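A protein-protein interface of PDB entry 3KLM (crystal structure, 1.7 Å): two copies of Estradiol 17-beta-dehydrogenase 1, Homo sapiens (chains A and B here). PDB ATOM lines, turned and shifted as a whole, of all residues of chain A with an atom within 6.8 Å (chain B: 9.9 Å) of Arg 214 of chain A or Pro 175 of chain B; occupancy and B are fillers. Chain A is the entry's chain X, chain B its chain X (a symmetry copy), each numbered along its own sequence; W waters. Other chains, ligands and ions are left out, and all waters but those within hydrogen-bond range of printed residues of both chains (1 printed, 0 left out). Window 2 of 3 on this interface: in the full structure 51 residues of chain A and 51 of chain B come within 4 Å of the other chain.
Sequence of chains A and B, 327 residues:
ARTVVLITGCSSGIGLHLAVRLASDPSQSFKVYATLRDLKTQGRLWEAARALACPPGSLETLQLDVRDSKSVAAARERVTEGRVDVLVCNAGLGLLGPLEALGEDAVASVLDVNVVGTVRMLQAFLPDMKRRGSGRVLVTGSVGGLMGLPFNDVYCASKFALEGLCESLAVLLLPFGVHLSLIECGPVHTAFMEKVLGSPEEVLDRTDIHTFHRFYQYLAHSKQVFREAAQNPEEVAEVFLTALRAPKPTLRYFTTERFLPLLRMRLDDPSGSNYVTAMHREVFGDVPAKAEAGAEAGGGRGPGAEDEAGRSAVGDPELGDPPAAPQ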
ATOM      1  N   PHE A 151      36.689  16.697  16.383  1.00  0.00           N
ATOM      2  CA  PHE A 151      36.466  16.245  15.018  1.00  0.00           C
ATOM      3  C   PHE A 151      37.696  15.778  14.303  1.00  0.00           C
ATOM      4  O   PHE A 151      37.619  15.539  13.109  1.00  0.00           O
ATOM      5  CB  PHE A 151      35.716  17.290  14.145  1.00  0.00           C
ATOM      6  CG  PHE A 151      34.398  17.690  14.756  1.00  0.00           C
ATOM      7  CD1 PHE A 151      33.327  16.833  14.688  1.00  0.00           C
ATOM      8  CD2 PHE A 151      34.275  18.893  15.468  1.00  0.00           C
ATOM      9  CE1 PHE A 151      32.116  17.165  15.268  1.00  0.00           C
ATOM     10  CE2 PHE A 151      33.054  19.224  16.057  1.00  0.00           C
ATOM     11  CZ  PHE A 151      31.989  18.382  15.953  1.00  0.00           C
ATOM     12  N   ILE A 209      21.948  17.054  14.157  1.00  0.00           N
ATOM     13  CA  ILE A 209      22.040  18.451  13.787  1.00  0.00           C
ATOM     14  C   ILE A 209      22.920  19.262  14.728  1.00  0.00           C
ATOM     15  O   ILE A 209      23.538  20.234  14.320  1.00  0.00           O
ATOM     16  CB  ILE A 209      20.587  19.098  13.731  1.00  0.00           C
ATOM     17  CG1 ILE A 209      20.650  20.490  13.131  1.00  0.00           C
ATOM     18  CG2 ILE A 209      19.910  19.086  15.100  1.00  0.00           C
ATOM     19  CD1 ILE A 209      21.296  20.520  11.760  1.00  0.00           C
ATOM     20  N   HIS A 210      22.946  18.866  15.987  1.00  0.00           N
ATOM     21  CA  HIS A 210      23.699  19.582  17.000  1.00  0.00           C
ATOM     22  C   HIS A 210      25.207  19.323  16.838  1.00  0.00           C
ATOM     23  O   HIS A 210      25.999  20.239  16.912  1.00  0.00           O
ATOM     24  CB  HIS A 210      23.211  19.162  18.371  1.00  0.00           C
ATOM     25  CG  HIS A 210      21.729  19.305  18.518  1.00  0.00           C
ATOM     26  ND1 HIS A 210      21.115  20.543  18.552  1.00  0.00           N
ATOM     27  CD2 HIS A 210      20.734  18.385  18.570  1.00  0.00           C
ATOM     28  CE1 HIS A 210      19.805  20.377  18.661  1.00  0.00           C
ATOM     29  NE2 HIS A 210      19.545  19.079  18.647  1.00  0.00           N
ATOM     30  N   THR A 211      25.568  18.067  16.628  1.00  0.00           N
ATOM     31  CA  THR A 211      26.961  17.757  16.274  1.00  0.00           C
ATOM     32  C   THR A 211      27.344  18.438  14.958  1.00  0.00           C
ATOM     33  O   THR A 211      28.442  19.023  14.820  1.00  0.00           O
ATOM     34  CB  THR A 211      27.154  16.222  16.141  1.00  0.00           C
ATOM     35  OG1 THR A 211      26.764  15.589  17.367  1.00  0.00           O
ATOM     36  CG2 THR A 211      28.639  15.937  15.824  1.00  0.00           C
ATOM     37  N   PHE A 212      26.457  18.373  13.964  1.00  0.00           N
ATOM     38  CA  PHE A 212      26.705  19.033  12.681  1.00  0.00           C
ATOM     39  C   PHE A 212      27.041  20.527  12.863  1.00  0.00           C
ATOM     40  O   PHE A 212      28.009  21.039  12.294  1.00  0.00           O
ATOM     41  CB  PHE A 212      25.493  18.894  11.763  1.00  0.00           C
ATOM     42  CG  PHE A 212      25.761  19.336  10.368  1.00  0.00           C
ATOM     43  CD1 PHE A 212      26.326  18.442   9.435  1.00  0.00           C
ATOM     44  CD2 PHE A 212      25.518  20.656   9.979  1.00  0.00           C
ATOM     45  CE1 PHE A 212      26.614  18.844   8.116  1.00  0.00           C
ATOM     46  CE2 PHE A 212      25.794  21.065   8.672  1.00  0.00           C
ATOM     47  CZ  PHE A 212      26.344  20.146   7.732  1.00  0.00           C
ATOM     48  N   HIS A 213      26.270  21.209  13.692  1.00  0.00           N
ATOM     49  CA  HIS A 213      26.549  22.597  13.988  1.00  0.00           C
ATOM     50  C   HIS A 213      27.876  22.833  14.709  1.00  0.00           C
ATOM     51  O   HIS A 213      28.598  23.800  14.427  1.00  0.00           O
ATOM     52  CB  HIS A 213      25.403  23.189  14.786  1.00  0.00           C
ATOM     53  CG  HIS A 213      25.645  24.598  15.227  1.00  0.00           C
ATOM     54  ND1 HIS A 213      26.025  24.917  16.516  1.00  0.00           N
ATOM     55  CD2 HIS A 213      25.560  25.768  14.555  1.00  0.00           C
ATOM     56  CE1 HIS A 213      26.168  26.228  16.619  1.00  0.00           C
ATOM     57  NE2 HIS A 213      25.890  26.768  15.444  1.00  0.00           N
ATOM     58  N   ARG A 214      28.210  21.961  15.656  1.00  0.00           N
ATOM     59  CA  ARG A 214      29.506  22.045  16.329  1.00  0.00           C
ATOM     60  C   ARG A 214      30.643  21.824  15.306  1.00  0.00           C
ATOM     61  O   ARG A 214      31.691  22.459  15.365  1.00  0.00           O
ATOM     62  CB  ARG A 214      29.574  20.960  17.396  1.00  0.00           C
ATOM     63  CG  ARG A 214      28.589  21.095  18.547  1.00  0.00           C
ATOM     64  CD  ARG A 214      29.049  22.177  19.473  1.00  0.00           C
ATOM     65  NE  ARG A 214      28.148  22.344  20.629  1.00  0.00           N
ATOM     66  CZ  ARG A 214      28.221  23.382  21.464  1.00  0.00           C
ATOM     67  NH1 ARG A 214      29.154  24.318  21.272  1.00  0.00           N
ATOM     68  NH2 ARG A 214      27.378  23.481  22.492  1.00  0.00           N
ATOM     69  N   PHE A 215      30.403  20.964  14.315  1.00  0.00           N
ATOM     70  CA  PHE A 215      31.414  20.721  13.280  1.00  0.00           C
ATOM     71  C   PHE A 215      31.704  22.004  12.514  1.00  0.00           C
ATOM     72  O   PHE A 215      32.835  22.321  12.210  1.00  0.00           O
ATOM     73  CB  PHE A 215      30.956  19.555  12.364  1.00  0.00           C
ATOM     74  CG  PHE A 215      31.997  19.100  11.333  1.00  0.00           C
ATOM     75  CD1 PHE A 215      33.350  18.994  11.641  1.00  0.00           C
ATOM     76  CD2 PHE A 215      31.593  18.705  10.060  1.00  0.00           C
ATOM     77  CE1 PHE A 215      34.302  18.582  10.667  1.00  0.00           C
ATOM     78  CE2 PHE A 215      32.541  18.258   9.095  1.00  0.00           C
ATOM     79  CZ  PHE A 215      33.892  18.198   9.401  1.00  0.00           C
ATOM     80  N   TYR A 216      30.657  22.776  12.211  1.00  0.00           N
ATOM     81  CA  TYR A 216      30.775  23.993  11.457  1.00  0.00           C
ATOM     82  C   TYR A 216      31.564  24.944  12.283  1.00  0.00           C
ATOM     83  O   TYR A 216      32.426  25.621  11.749  1.00  0.00           O
ATOM     84  CB  TYR A 216      29.370  24.630  11.269  1.00  0.00           C
ATOM     85  CG  TYR A 216      29.438  25.969  10.565  1.00  0.00           C
ATOM     86  CD1 TYR A 216      29.645  27.168  11.294  1.00  0.00           C
ATOM     87  CD2 TYR A 216      29.292  26.038   9.177  1.00  0.00           C
ATOM     88  CE1 TYR A 216      29.750  28.395  10.633  1.00  0.00           C
ATOM     89  CE2 TYR A 216      29.376  27.245   8.519  1.00  0.00           C
ATOM     90  CZ  TYR A 216      29.597  28.405   9.248  1.00  0.00           C
ATOM     91  OH  TYR A 216      29.654  29.578   8.548  1.00  0.00           O
ATOM     92  N   GLN A 217      31.261  25.006  13.568  1.00  0.00           N
ATOM     93  CA  GLN A 217      31.961  25.937  14.441  1.00  0.00           C
ATOM     94  C   GLN A 217      33.451  25.607  14.476  1.00  0.00           C
ATOM     95  O   GLN A 217      34.333  26.508  14.477  1.00  0.00           O
ATOM     96  CB  GLN A 217      31.470  25.856  15.853  1.00  0.00           C
ATOM     97  CG  GLN A 217      30.106  26.506  16.094  1.00  0.00           C
ATOM     98  CD  GLN A 217      29.671  26.341  17.522  1.00  0.00           C
ATOM     99  OE1 GLN A 217      29.306  25.255  17.964  1.00  0.00           O
ATOM    100  NE2 GLN A 217      29.748  27.425  18.283  1.00  0.00           N
ATOM    101  N   TYR A 218      33.712  24.310  14.559  1.00  0.00           N
ATOM    102  CA  TYR A 218      35.124  23.848  14.578  1.00  0.00           C
ATOM    103  C   TYR A 218      35.821  24.277  13.269  1.00  0.00           C
ATOM    104  O   TYR A 218      36.910  24.886  13.296  1.00  0.00           O
ATOM    105  CB  TYR A 218      35.231  22.327  14.847  1.00  0.00           C
ATOM    106  CG  TYR A 218      36.631  21.884  14.488  1.00  0.00           C
ATOM    107  CD1 TYR A 218      37.690  22.067  15.371  1.00  0.00           C
ATOM    108  CD2 TYR A 218      36.895  21.405  13.217  1.00  0.00           C
ATOM    109  CE1 TYR A 218      38.994  21.714  14.996  1.00  0.00           C
ATOM    110  CE2 TYR A 218      38.187  21.078  12.833  1.00  0.00           C
ATOM    111  CZ  TYR A 218      39.217  21.230  13.739  1.00  0.00           C
ATOM    112  OH  TYR A 218      40.499  20.905  13.323  1.00  0.00           O
ATOM    113  N   LEU A 219      35.187  24.001  12.119  1.00  0.00           N
ATOM    114  CA  LEU A 219      35.723  24.406  10.840  1.00  0.00           C
ATOM    115  C   LEU A 219      35.974  25.912  10.740  1.00  0.00           C
ATOM    116  O   LEU A 219      37.009  26.344  10.238  1.00  0.00           O
ATOM    117  CB  LEU A 219      34.821  23.941   9.712  1.00  0.00           C
ATOM    118  CG  LEU A 219      34.731  22.434   9.540  1.00  0.00           C
ATOM    119  CD1 LEU A 219      33.741  22.187   8.482  1.00  0.00           C
ATOM    120  CD2 LEU A 219      36.115  21.759   9.175  1.00  0.00           C
ATOM    121  N   HIS A 280      37.841  23.476  24.723  1.00  0.00           N
ATOM    122  CA  HIS A 280      36.437  23.638  24.390  1.00  0.00           C
ATOM    123  C   HIS A 280      36.130  25.144  24.208  1.00  0.00           C
ATOM    124  O   HIS A 280      35.516  25.541  23.216  1.00  0.00           O
ATOM    125  CB  HIS A 280      35.512  23.055  25.446  1.00  0.00           C
ATOM    126  CG  HIS A 280      34.072  23.136  25.063  1.00  0.00           C
ATOM    127  ND1 HIS A 280      33.308  24.264  25.293  1.00  0.00           N
ATOM    128  CD2 HIS A 280      33.275  22.264  24.403  1.00  0.00           C
ATOM    129  CE1 HIS A 280      32.093  24.067  24.819  1.00  0.00           C
ATOM    130  NE2 HIS A 280      32.045  22.863  24.272  1.00  0.00           N
ATOM    131  N   VAL A 283      37.773  26.597  20.934  1.00  0.00           N
ATOM    132  CA  VAL A 283      37.086  26.234  19.671  1.00  0.00           C
ATOM    133  C   VAL A 283      35.632  26.708  19.610  1.00  0.00           C
ATOM    134  O   VAL A 283      35.162  27.156  18.554  1.00  0.00           O
ATOM    135  CB  VAL A 283      37.119  24.684  19.414  1.00  0.00           C
ATOM    136  CG1 VAL A 283      36.338  24.300  18.160  1.00  0.00           C
ATOM    137  CG2 VAL A 283      38.532  24.215  19.293  1.00  0.00           C
ATOM    138  N   PHE A 284      34.920  26.566  20.719  1.00  0.00           N
ATOM    139  CA  PHE A 284      33.489  26.792  20.719  1.00  0.00           C
ATOM    140  C   PHE A 284      33.174  28.093  21.461  1.00  0.00           C
ATOM    141  O   PHE A 284      34.073  28.762  22.007  1.00  0.00           O
ATOM    142  CB  PHE A 284      32.735  25.589  21.308  1.00  0.00           C
ATOM    143  CG  PHE A 284      33.009  24.295  20.581  1.00  0.00           C
ATOM    144  CD1 PHE A 284      32.578  24.113  19.274  1.00  0.00           C
ATOM    145  CD2 PHE A 284      33.749  23.279  21.184  1.00  0.00           C
ATOM    146  CE1 PHE A 284      32.846  22.935  18.582  1.00  0.00           C
ATOM    147  CE2 PHE A 284      34.027  22.088  20.493  1.00  0.00           C
ATOM    148  CZ  PHE A 284      33.573  21.924  19.192  1.00  0.00           C
ATOM    149  N   MET B 129      23.499   7.952  23.332  1.00  0.00           N
ATOM    150  CA  MET B 129      23.892   8.723  24.515  1.00  0.00           C
ATOM    151  C   MET B 129      23.760  10.239  24.283  1.00  0.00           C
ATOM    152  O   MET B 129      23.273  11.011  25.160  1.00  0.00           O
ATOM    153  CB  MET B 129      25.328   8.373  24.903  1.00  0.00           C
ATOM    154  CG  MET B 129      25.452   7.006  25.482  1.00  0.00           C
ATOM    155  SD  MET B 129      27.165   6.700  26.064  1.00  0.00           S
ATOM    156  CE  MET B 129      27.007   5.021  26.661  1.00  0.00           C
ATOM    157  N   LYS B 130      24.183  10.680  23.104  1.00  0.00           N
ATOM    158  CA  LYS B 130      24.149  12.122  22.781  1.00  0.00           C
ATOM    159  C   LYS B 130      22.695  12.564  22.686  1.00  0.00           C
ATOM    160  O   LYS B 130      22.366  13.678  23.090  1.00  0.00           O
ATOM    161  CB  LYS B 130      24.847  12.416  21.449  1.00  0.00           C
ATOM    162  CG  LYS B 130      26.362  12.269  21.478  1.00  0.00           C
ATOM    163  CD  LYS B 130      26.881  12.046  20.067  1.00  0.00           C
ATOM    164  CE  LYS B 130      27.475  13.308  19.493  1.00  0.00           C
ATOM    165  NZ  LYS B 130      27.821  13.124  18.047  1.00  0.00           N
ATOM    166  N   ARG B 131      21.850  11.673  22.172  1.00  0.00           N
ATOM    167  CA  ARG B 131      20.420  11.949  21.993  1.00  0.00           C
ATOM    168  C   ARG B 131      19.743  12.109  23.350  1.00  0.00           C
ATOM    169  O   ARG B 131      18.962  13.052  23.552  1.00  0.00           O
ATOM    170  CB  ARG B 131      19.752  10.838  21.184  1.00  0.00           C
ATOM    171  CG  ARG B 131      18.243  10.935  21.143  1.00  0.00           C
ATOM    172  CD  ARG B 131      17.583   9.715  20.471  1.00  0.00           C
ATOM    173  NE  ARG B 131      17.282   8.588  21.378  1.00  0.00           N
ATOM    174  CZ  ARG B 131      16.431   8.615  22.416  1.00  0.00           C
ATOM    175  NH1 ARG B 131      15.800   9.736  22.767  1.00  0.00           N
ATOM    176  NH2 ARG B 131      16.230   7.510  23.134  1.00  0.00           N
ATOM    177  N   ARG B 132      20.057  11.207  24.277  1.00  0.00           N
ATOM    178  CA  ARG B 132      19.479  11.216  25.627  1.00  0.00           C
ATOM    179  C   ARG B 132      20.036  12.342  26.439  1.00  0.00           C
ATOM    180  O   ARG B 132      19.495  12.671  27.496  1.00  0.00           O
ATOM    181  CB  ARG B 132      19.775   9.923  26.382  1.00  0.00           C
ATOM    182  CG  ARG B 132      19.000   8.748  25.880  1.00  0.00           C
ATOM    183  CD  ARG B 132      19.200   7.507  26.730  1.00  0.00           C
ATOM    184  NE  ARG B 132      18.606   6.339  26.062  1.00  0.00           N
ATOM    185  CZ  ARG B 132      17.356   5.900  26.248  1.00  0.00           C
ATOM    186  NH1 ARG B 132      16.535   6.508  27.100  1.00  0.00           N
ATOM    187  NH2 ARG B 132      16.921   4.837  25.583  1.00  0.00           N
ATOM    188  N   GLY B 133      21.140  12.906  25.975  1.00  0.00           N
ATOM    189  CA  GLY B 133      21.917  13.844  26.792  1.00  0.00           C
ATOM    190  C   GLY B 133      22.469  13.222  28.062  1.00  0.00           C
ATOM    191  O   GLY B 133      22.665  13.917  29.068  1.00  0.00           O
ATOM    192  N   SER B 134      22.714  11.912  28.038  1.00  0.00           N
ATOM    193  CA  SER B 134      23.383  11.274  29.180  1.00  0.00           C
ATOM    194  C   SER B 134      24.046   9.899  28.884  1.00  0.00           C
ATOM    195  O   SER B 134      23.655   9.142  27.972  1.00  0.00           O
ATOM    196  CB  SER B 134      22.464  11.202  30.412  1.00  0.00           C
ATOM    197  OG  SER B 134      21.677  10.025  30.370  1.00  0.00           O
ATOM    198  N   SER B 168      40.237  14.033  22.240  1.00  0.00           N
ATOM    199  CA  SER B 168      39.566  14.696  21.127  1.00  0.00           C
ATOM    200  C   SER B 168      38.062  14.659  21.325  1.00  0.00           C
ATOM    201  O   SER B 168      37.392  15.729  21.232  1.00  0.00           O
ATOM    202  CB  SER B 168      39.987  14.046  19.781  1.00  0.00           C
ATOM    203  OG  SER B 168      41.388  14.197  19.501  1.00  0.00           O
ATOM    204  N   LEU B 169      37.514  13.465  21.567  1.00  0.00           N
ATOM    205  CA  LEU B 169      36.075  13.260  21.820  1.00  0.00           C
ATOM    206  C   LEU B 169      35.560  14.026  23.030  1.00  0.00           C
ATOM    207  O   LEU B 169      34.453  14.633  22.946  1.00  0.00           O
ATOM    208  CB  LEU B 169      35.707  11.765  21.957  1.00  0.00           C
ATOM    209  CG  LEU B 169      35.635  10.894  20.711  1.00  0.00           C
ATOM    210  CD1 LEU B 169      35.648   9.471  21.160  1.00  0.00           C
ATOM    211  CD2 LEU B 169      34.384  11.223  19.940  1.00  0.00           C
ATOM    212  N   ALA B 170      36.334  14.041  24.114  1.00  0.00           N
ATOM    213  CA  ALA B 170      35.920  14.744  25.347  1.00  0.00           C
ATOM    214  C   ALA B 170      35.726  16.256  25.135  1.00  0.00           C
ATOM    215  O   ALA B 170      34.830  16.874  25.766  1.00  0.00           O
ATOM    216  CB  ALA B 170      36.916  14.512  26.451  1.00  0.00           C
ATOM    217  N   VAL B 171      36.557  16.846  24.278  1.00  0.00           N
ATOM    218  CA  VAL B 171      36.445  18.294  23.975  1.00  0.00           C
ATOM    219  C   VAL B 171      35.059  18.559  23.363  1.00  0.00           C
ATOM    220  O   VAL B 171      34.427  19.594  23.626  1.00  0.00           O
ATOM    221  CB  VAL B 171      37.577  18.755  23.034  1.00  0.00           C
ATOM    222  CG1 VAL B 171      37.330  20.180  22.504  1.00  0.00           C
ATOM    223  CG2 VAL B 171      38.927  18.699  23.735  1.00  0.00           C
ATOM    224  N   LEU B 172      34.568  17.622  22.553  1.00  0.00           N
ATOM    225  CA  LEU B 172      33.268  17.769  21.910  1.00  0.00           C
ATOM    226  C   LEU B 172      32.080  17.396  22.788  1.00  0.00           C
ATOM    227  O   LEU B 172      31.055  18.093  22.767  1.00  0.00           O
ATOM    228  CB  LEU B 172      33.221  16.962  20.602  1.00  0.00           C
ATOM    229  CG  LEU B 172      31.859  16.873  19.923  1.00  0.00           C
ATOM    230  CD1 LEU B 172      31.371  18.253  19.405  1.00  0.00           C
ATOM    231  CD2 LEU B 172      31.884  15.842  18.821  1.00  0.00           C
ATOM    232  N   LEU B 173      32.206  16.295  23.534  1.00  0.00           N
ATOM    233  CA  LEU B 173      31.085  15.710  24.267  1.00  0.00           C
ATOM    234  C   LEU B 173      30.651  16.514  25.509  1.00  0.00           C
ATOM    235  O   LEU B 173      29.568  16.295  26.033  1.00  0.00           O
ATOM    236  CB  LEU B 173      31.424  14.292  24.696  1.00  0.00           C
ATOM    237  CG  LEU B 173      31.591  13.233  23.617  1.00  0.00           C
ATOM    238  CD1 LEU B 173      32.196  11.988  24.257  1.00  0.00           C
ATOM    239  CD2 LEU B 173      30.283  12.937  22.907  1.00  0.00           C
ATOM    240  N   LEU B 174      31.512  17.414  25.973  1.00  0.00           N
ATOM    241  CA  LEU B 174      31.275  18.204  27.177  1.00  0.00           C
ATOM    242  C   LEU B 174      29.837  18.785  27.212  1.00  0.00           C
ATOM    243  O   LEU B 174      29.046  18.399  28.093  1.00  0.00           O
ATOM    244  CB  LEU B 174      32.371  19.294  27.321  1.00  0.00           C
ATOM    245  CG  LEU B 174      32.635  20.018  28.657  1.00  0.00           C
ATOM    246  CD1 LEU B 174      32.821  19.023  29.808  1.00  0.00           C
ATOM    247  CD2 LEU B 174      33.819  20.999  28.595  1.00  0.00           C
ATOM    248  N   PRO B 175      29.462  19.655  26.234  1.00  0.00           N
ATOM    249  CA  PRO B 175      28.076  20.190  26.271  1.00  0.00           C
ATOM    250  C   PRO B 175      26.945  19.180  26.025  1.00  0.00           C
ATOM    251  O   PRO B 175      25.775  19.533  26.221  1.00  0.00           O
ATOM    252  CB  PRO B 175      28.083  21.246  25.149  1.00  0.00           C
ATOM    253  CG  PRO B 175      29.139  20.764  24.182  1.00  0.00           C
ATOM    254  CD  PRO B 175      30.215  20.221  25.093  1.00  0.00           C
ATOM    255  N   PHE B 176      27.265  17.950  25.606  1.00  0.00           N
ATOM    256  CA  PHE B 176      26.237  16.932  25.375  1.00  0.00           C
ATOM    257  C   PHE B 176      25.823  16.194  26.652  1.00  0.00           C
ATOM    258  O   PHE B 176      24.912  15.371  26.611  1.00  0.00           O
ATOM    259  CB  PHE B 176      26.682  15.896  24.346  1.00  0.00           C
ATOM    260  CG  PHE B 176      26.638  16.378  22.923  1.00  0.00           C
ATOM    261  CD1 PHE B 176      27.649  17.176  22.412  1.00  0.00           C
ATOM    262  CD2 PHE B 176      25.593  16.015  22.098  1.00  0.00           C
ATOM    263  CE1 PHE B 176      27.615  17.625  21.087  1.00  0.00           C
ATOM    264  CE2 PHE B 176      25.556  16.453  20.773  1.00  0.00           C
ATOM    265  CZ  PHE B 176      26.578  17.259  20.278  1.00  0.00           C
ATOM    266  N   GLY B 177      26.485  16.455  27.774  1.00  0.00           N
ATOM    267  CA  GLY B 177      26.208  15.658  28.989  1.00  0.00           C
ATOM    268  C   GLY B 177      26.680  14.189  29.015  1.00  0.00           C
ATOM    269  O   GLY B 177      26.289  13.422  29.892  1.00  0.00           O
ATOM    270  N   VAL B 178      27.528  13.800  28.062  1.00  0.00           N
ATOM    271  CA  VAL B 178      28.041  12.436  27.977  1.00  0.00           C
ATOM    272  C   VAL B 178      29.486  12.578  28.456  1.00  0.00           C
ATOM    273  O   VAL B 178      30.215  13.449  27.975  1.00  0.00           O
ATOM    274  CB  VAL B 178      27.966  11.908  26.508  1.00  0.00           C
ATOM    275  CG1 VAL B 178      28.587  10.500  26.367  1.00  0.00           C
ATOM    276  CG2 VAL B 178      26.507  11.858  26.006  1.00  0.00           C
ATOM    277  N   HIS B 179      29.888  11.763  29.435  1.00  0.00           N
ATOM    278  CA  HIS B 179      31.176  11.935  30.105  1.00  0.00           C
ATOM    279  C   HIS B 179      32.065  10.756  29.747  1.00  0.00           C
ATOM    280  O   HIS B 179      31.627   9.625  29.849  1.00  0.00           O
ATOM    281  CB  HIS B 179      30.974  11.976  31.622  1.00  0.00           C
ATOM    282  CG  HIS B 179      29.955  12.974  32.071  1.00  0.00           C
ATOM    283  ND1 HIS B 179      30.237  14.314  32.193  1.00  0.00           N
ATOM    284  CD2 HIS B 179      28.654  12.828  32.411  1.00  0.00           C
ATOM    285  CE1 HIS B 179      29.156  14.956  32.597  1.00  0.00           C
ATOM    286  NE2 HIS B 179      28.181  14.077  32.736  1.00  0.00           N
ATOM    287  N   LYS B 248      30.772  15.016  38.452  1.00  0.00           N
ATOM    288  CA  LYS B 248      31.432  15.534  37.229  1.00  0.00           C
ATOM    289  C   LYS B 248      32.789  14.851  37.007  1.00  0.00           C
ATOM    290  O   LYS B 248      33.812  15.287  37.552  1.00  0.00           O
ATOM    291  CB  LYS B 248      31.645  17.051  37.269  1.00  0.00           C
ATOM    292  CG  LYS B 248      31.408  17.774  35.891  1.00  0.00           C
ATOM    293  CD  LYS B 248      32.361  17.335  34.715  1.00  0.00           C
ATOM    294  CE  LYS B 248      33.440  18.393  34.369  1.00  0.00           C
ATOM    295  NZ  LYS B 248      34.695  18.274  35.190  1.00  0.00           N
HETATM  296  O   HOH W   1      35.697  15.128  18.658  1.00  0.00           O
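Of the printed residues of chain B, Phe 151 of chain A touches Leu 172 (3.5 Å). Of chain B, only Leu 172 (3.8 Å) and Pro 175 (3.5 Å) come within 4 Å of Arg 214 of chain A. No residue of chain B comes within 4 Å of Gln 217 of chain A. Printed residues of chain B within 4 Å of His 280 of chain A: Val 171 and Pro 175. Printed residues of chain A within 4 Å of Val 171 of chain B: His 280. Of the printed residues of chain A, Leu 172 of chain B touches Phe 151 and Arg 214. Pro 175 of chain B touches just these residues of chain A: Arg 214 (3.5 Å) and His 280 (3.3 Å). The nearest residue of chain A that does not touch Pro 175 of chain B is Phe 284 of chain A (6.0 Å).
No position is printed for both chains. Of the 7 pairs that touch across the chains among the printed residues, none has its exchanged pair printed and touching as well.
CZ of Phe 151 of chain A touches CD1 of Leu 172 of chain B, at 3.5 Å. OG1 of Thr 211 of chain A touches CZ of Phe 176 of chain B, 3.4 Å away. Arg 214 of chain A touches Leu 172 of chain B. NH2 of Arg 214 of chain A touches CB of Pro 175 of chain B, at 3.5 Å. CD2 of His 280 of chain A touches O of Val 171 of chain B, at 3.0 Å. His 280 of chain A touches Pro 175 of chain B.
Water W1 bridges the backbone NH of Phe 151 of chain A (2.9 Å) and the backbone carbonyl oxygen of Ser 168 of chain B (3.1 Å).
The side-chain hydroxyl (OG1) of Thr 211 of chain A sits at hydrogen-bond distance from the side-chain amino group (NZ) of Lys 130 of chain B, 2.8 Å away.
Hydrophobic or aromatic side chains of chain B within 4 Å of the printed part of chain A: Leu 172, Pro 175 and Phe 176. Of the 15 printed residues of chain A, 4 touch a printed residue of chain B. Hydrophobic or aromatic side chains of chain A within 4 Å of the printed part of chain B: Phe 151 and His 280. Among the printed residues, no Asp or Glu carboxylate lies within 4 Å of a Lys or Arg side-chain nitrogen of the other chain.
The guanidinium group (NH1) of Arg 214 of chain A lies close to the side-chain amide oxygen (OE1) of Gln 217 of chain A.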
